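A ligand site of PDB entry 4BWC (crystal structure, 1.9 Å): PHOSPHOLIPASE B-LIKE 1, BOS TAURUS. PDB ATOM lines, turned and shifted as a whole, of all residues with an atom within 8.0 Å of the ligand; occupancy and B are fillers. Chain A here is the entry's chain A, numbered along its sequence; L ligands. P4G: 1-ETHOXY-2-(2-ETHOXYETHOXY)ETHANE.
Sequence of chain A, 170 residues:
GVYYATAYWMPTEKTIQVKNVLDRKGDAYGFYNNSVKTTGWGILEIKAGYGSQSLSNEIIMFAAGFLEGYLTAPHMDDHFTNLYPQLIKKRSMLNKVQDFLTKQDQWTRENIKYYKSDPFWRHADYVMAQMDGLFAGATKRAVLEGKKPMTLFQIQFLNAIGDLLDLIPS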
ATOM      1  N   THR A   6      -5.965 -14.216 -10.364  1.00  0.00           N
ATOM      2  CA  THR A   6      -5.389 -13.869 -11.626  1.00  0.00           C
ATOM      3  C   THR A   6      -6.260 -14.356 -12.735  1.00  0.00           C
ATOM      4  O   THR A   6      -6.720 -15.504 -12.726  1.00  0.00           O
ATOM      5  CB  THR A   6      -3.913 -14.451 -11.756  1.00  0.00           C
ATOM      6  OG1 THR A   6      -3.127 -14.100 -10.617  1.00  0.00           O
ATOM      7  CG2 THR A   6      -3.216 -13.954 -12.889  1.00  0.00           C
ATOM      8  N   ALA A   7      -6.479 -13.487 -13.705  1.00  0.00           N
ATOM      9  CA  ALA A   7      -7.249 -13.826 -14.860  1.00  0.00           C
ATOM     10  C   ALA A   7      -6.321 -13.993 -16.057  1.00  0.00           C
ATOM     11  O   ALA A   7      -5.351 -13.243 -16.180  1.00  0.00           O
ATOM     12  CB  ALA A   7      -8.232 -12.699 -15.172  1.00  0.00           C
ATOM     13  N   TYR A   8      -6.670 -14.900 -16.957  1.00  0.00           N
ATOM     14  CA  TYR A   8      -5.941 -15.158 -18.223  1.00  0.00           C
ATOM     15  C   TYR A   8      -6.875 -15.104 -19.380  1.00  0.00           C
ATOM     16  O   TYR A   8      -7.860 -15.849 -19.448  1.00  0.00           O
ATOM     17  CB  TYR A   8      -5.259 -16.553 -18.217  1.00  0.00           C
ATOM     18  CG  TYR A   8      -4.406 -16.774 -16.988  1.00  0.00           C
ATOM     19  CD1 TYR A   8      -4.962 -17.215 -15.813  1.00  0.00           C
ATOM     20  CD2 TYR A   8      -3.059 -16.486 -17.012  1.00  0.00           C
ATOM     21  CE1 TYR A   8      -4.200 -17.368 -14.702  1.00  0.00           C
ATOM     22  CE2 TYR A   8      -2.281 -16.655 -15.897  1.00  0.00           C
ATOM     23  CZ  TYR A   8      -2.833 -17.094 -14.755  1.00  0.00           C
ATOM     24  OH  TYR A   8      -2.041 -17.260 -13.611  1.00  0.00           O
ATOM     25  N   TRP A   9      -6.571 -14.266 -20.340  1.00  0.00           N
ATOM     26  CA  TRP A   9      -7.323 -14.290 -21.585  1.00  0.00           C
ATOM     27  C   TRP A   9      -6.832 -15.468 -22.399  1.00  0.00           C
ATOM     28  O   TRP A   9      -5.632 -15.635 -22.601  1.00  0.00           O
ATOM     29  CB  TRP A   9      -7.121 -12.976 -22.327  1.00  0.00           C
ATOM     30  CG  TRP A   9      -7.793 -12.836 -23.654  1.00  0.00           C
ATOM     31  CD1 TRP A   9      -7.166 -12.671 -24.885  1.00  0.00           C
ATOM     32  CD2 TRP A   9      -9.224 -12.776 -23.953  1.00  0.00           C
ATOM     33  NE1 TRP A   9      -8.077 -12.551 -25.876  1.00  0.00           N
ATOM     34  CE2 TRP A   9      -9.329 -12.604 -25.399  1.00  0.00           C
ATOM     35  CE3 TRP A   9     -10.411 -12.846 -23.192  1.00  0.00           C
ATOM     36  CZ2 TRP A   9     -10.548 -12.515 -26.054  1.00  0.00           C
ATOM     37  CZ3 TRP A   9     -11.631 -12.760 -23.857  1.00  0.00           C
ATOM     38  CH2 TRP A   9     -11.707 -12.572 -25.237  1.00  0.00           C
ATOM     39  N   MET A  10      -7.783 -16.292 -22.855  1.00  0.00           N
ATOM     40  CA  MET A  10      -7.505 -17.415 -23.780  1.00  0.00           C
ATOM     41  C   MET A  10      -7.990 -16.924 -25.142  1.00  0.00           C
ATOM     42  O   MET A  10      -9.183 -16.998 -25.412  1.00  0.00           O
ATOM     43  CB  MET A  10      -8.305 -18.691 -23.402  1.00  0.00           C
ATOM     44  CG  MET A  10      -8.390 -19.133 -21.937  1.00  0.00           C
ATOM     45  SD  MET A  10      -6.795 -19.310 -21.122  1.00  0.00           S
ATOM     46  CE  MET A  10      -7.090 -20.701 -20.020  1.00  0.00           C
ATOM     47  N   GLN A  17      -9.982 -17.392 -18.054  1.00  0.00           N
ATOM     48  CA  GLN A  17     -10.025 -18.338 -16.960  1.00  0.00           C
ATOM     49  C   GLN A  17      -9.347 -17.664 -15.786  1.00  0.00           C
ATOM     50  O   GLN A  17      -8.381 -16.898 -15.966  1.00  0.00           O
ATOM     51  CB  GLN A  17      -9.324 -19.678 -17.352  1.00  0.00           C
ATOM     52  CG  GLN A  17      -8.855 -20.565 -16.180  1.00  0.00           C
ATOM     53  CD  GLN A  17      -7.755 -21.600 -16.540  1.00  0.00           C
ATOM     54  OE1 GLN A  17      -7.776 -22.228 -17.614  1.00  0.00           O
ATOM     55  NE2 GLN A  17      -6.804 -21.804 -15.621  1.00  0.00           N
ATOM     56  N   VAL A  18      -9.804 -17.979 -14.577  1.00  0.00           N
ATOM     57  CA  VAL A  18      -9.241 -17.406 -13.371  1.00  0.00           C
ATOM     58  C   VAL A  18      -8.600 -18.447 -12.504  1.00  0.00           C
ATOM     59  O   VAL A  18      -9.087 -19.553 -12.474  1.00  0.00           O
ATOM     60  CB  VAL A  18     -10.326 -16.703 -12.517  1.00  0.00           C
ATOM     61  CG1 VAL A  18      -9.799 -16.393 -11.129  1.00  0.00           C
ATOM     62  CG2 VAL A  18     -10.697 -15.402 -13.145  1.00  0.00           C
ATOM     63  N   LYS A  19      -7.532 -18.094 -11.773  1.00  0.00           N
ATOM     64  CA  LYS A  19      -6.901 -18.976 -10.797  1.00  0.00           C
ATOM     65  C   LYS A  19      -6.738 -18.171  -9.561  1.00  0.00           C
ATOM     66  O   LYS A  19      -6.575 -16.924  -9.625  1.00  0.00           O
ATOM     67  CB  LYS A  19      -5.522 -19.505 -11.282  1.00  0.00           C
ATOM     68  CG  LYS A  19      -5.574 -20.417 -12.515  1.00  0.00           C
ATOM     69  CD  LYS A  19      -4.164 -20.884 -12.854  1.00  0.00           C
ATOM     70  CE  LYS A  19      -4.163 -22.264 -13.471  1.00  0.00           C
ATOM     71  NZ  LYS A  19      -2.819 -22.649 -13.945  1.00  0.00           N
ATOM     72  N   ASN A  20      -6.757 -18.862  -8.434  1.00  0.00           N
ATOM     73  CA  ASN A  20      -6.628 -18.215  -7.146  1.00  0.00           C
ATOM     74  C   ASN A  20      -5.227 -18.034  -6.614  1.00  0.00           C
ATOM     75  O   ASN A  20      -4.978 -18.213  -5.423  1.00  0.00           O
ATOM     76  CB  ASN A  20      -7.469 -18.881  -6.072  1.00  0.00           C
ATOM     77  CG  ASN A  20      -8.918 -18.938  -6.459  1.00  0.00           C
ATOM     78  OD1 ASN A  20      -9.563 -17.918  -6.676  1.00  0.00           O
ATOM     79  ND2 ASN A  20      -9.426 -20.146  -6.574  1.00  0.00           N
ATOM     80  N   VAL A  21      -4.340 -17.566  -7.482  1.00  0.00           N
ATOM     81  CA  VAL A  21      -2.991 -17.144  -7.075  1.00  0.00           C
ATOM     82  C   VAL A  21      -2.677 -15.712  -7.602  1.00  0.00           C
ATOM     83  O   VAL A  21      -3.345 -15.214  -8.515  1.00  0.00           O
ATOM     84  CB  VAL A  21      -1.956 -18.129  -7.613  1.00  0.00           C
ATOM     85  CG1 VAL A  21      -2.050 -19.461  -6.823  1.00  0.00           C
ATOM     86  CG2 VAL A  21      -2.168 -18.308  -9.105  1.00  0.00           C
ATOM     87  N   LEU A  22      -1.685 -15.074  -7.006  1.00  0.00           N
ATOM     88  CA  LEU A  22      -1.120 -13.860  -7.615  1.00  0.00           C
ATOM     89  C   LEU A  22      -0.015 -14.206  -8.605  1.00  0.00           C
ATOM     90  O   LEU A  22       1.096 -14.498  -8.201  1.00  0.00           O
ATOM     91  CB  LEU A  22      -0.589 -12.948  -6.513  1.00  0.00           C
ATOM     92  CG  LEU A  22      -0.024 -11.598  -6.986  1.00  0.00           C
ATOM     93  CD1 LEU A  22      -1.141 -10.604  -7.243  1.00  0.00           C
ATOM     94  CD2 LEU A  22       0.897 -11.138  -5.874  1.00  0.00           C
ATOM     95  N   ASP A  23      -0.309 -14.122  -9.888  1.00  0.00           N
ATOM     96  CA  ASP A  23       0.685 -14.379 -10.905  1.00  0.00           C
ATOM     97  C   ASP A  23       0.925 -13.175 -11.879  1.00  0.00           C
ATOM     98  O   ASP A  23       0.131 -12.911 -12.833  1.00  0.00           O
ATOM     99  CB  ASP A  23       0.302 -15.668 -11.660  1.00  0.00           C
ATOM    100  CG  ASP A  23       1.088 -15.869 -12.939  1.00  0.00           C
ATOM    101  OD1 ASP A  23       2.198 -15.305 -13.069  1.00  0.00           O
ATOM    102  OD2 ASP A  23       0.589 -16.562 -13.839  1.00  0.00           O
ATOM    103  N   LYS A  25       2.438 -12.731 -14.487  1.00  0.00           N
ATOM    104  CA  LYS A  25       2.403 -12.896 -15.970  1.00  0.00           C
ATOM    105  C   LYS A  25       0.983 -12.882 -16.445  1.00  0.00           C
ATOM    106  O   LYS A  25       0.747 -12.861 -17.672  1.00  0.00           O
ATOM    107  CB  LYS A  25       3.095 -14.235 -16.467  1.00  0.00           C
ATOM    108  CG  LYS A  25       4.350 -14.628 -15.698  1.00  0.00           C
ATOM    109  CD  LYS A  25       5.502 -13.714 -16.091  1.00  0.00           C
ATOM    110  CE  LYS A  25       6.842 -14.242 -15.623  1.00  0.00           C
ATOM    111  NZ  LYS A  25       7.826 -13.105 -15.586  1.00  0.00           N
ATOM    112  N   GLY A  26       0.043 -12.872 -15.481  1.00  0.00           N
ATOM    113  CA  GLY A  26      -1.399 -12.911 -15.811  1.00  0.00           C
ATOM    114  C   GLY A  26      -1.901 -11.633 -16.493  1.00  0.00           C
ATOM    115  O   GLY A  26      -1.236 -10.570 -16.411  1.00  0.00           O
HETATM  116  C8  P4G L   1      -3.996 -24.306 -16.612  1.00  0.00           C
HETATM  117  C7  P4G L   1      -3.773 -23.219 -17.674  1.00  0.00           C
HETATM  118  O4  P4G L   1      -4.083 -21.875 -17.195  1.00  0.00           O
HETATM  119  C6  P4G L   1      -3.420 -20.785 -17.848  1.00  0.00           C
HETATM  120  C5  P4G L   1      -2.166 -20.307 -17.069  1.00  0.00           C
HETATM  121  O3  P4G L   1      -2.064 -20.757 -15.683  1.00  0.00           O
HETATM  122  C4  P4G L   1      -0.783 -20.529 -15.049  1.00  0.00           C
HETATM  123  C3  P4G L   1      -0.814 -20.436 -13.517  1.00  0.00           C
HETATM  124  O2  P4G L   1      -0.528 -21.658 -12.789  1.00  0.00           O
HETATM  125  C2  P4G L   1      -0.939 -21.703 -11.407  1.00  0.00           C
HETATM  126  C1  P4G L   1       0.089 -22.386 -10.502  1.00  0.00           C
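Merely in contact with the ligand: Tyr 8 (3.4 Å).
Within 4 Å of the ligand: Tyr 8, Gln 17 and Lys 19.
The nearest printed residue that does not touch the ligand is Asp 23 (4.1 Å).
NZ of Lys 19 sits at hydrogen-bond distance from O3 of the ligand (2.7 Å).
NE2 of Gln 17 sits at hydrogen-bond distance from O4 of the ligand (3.1 Å).
The backbone carbonyl oxygen of Lys 19 is in hydrogen-bond range of the backbone NH of Thr 6, at 2.9 Å.
The backbone carbonyl oxygen (O) of Gln 17 lies within hydrogen-bond range of the backbone NH (N) of Tyr 8.
OH of Tyr 8 is in hydrogen-bond range of OD2 of Asp 23 (2.7 Å).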
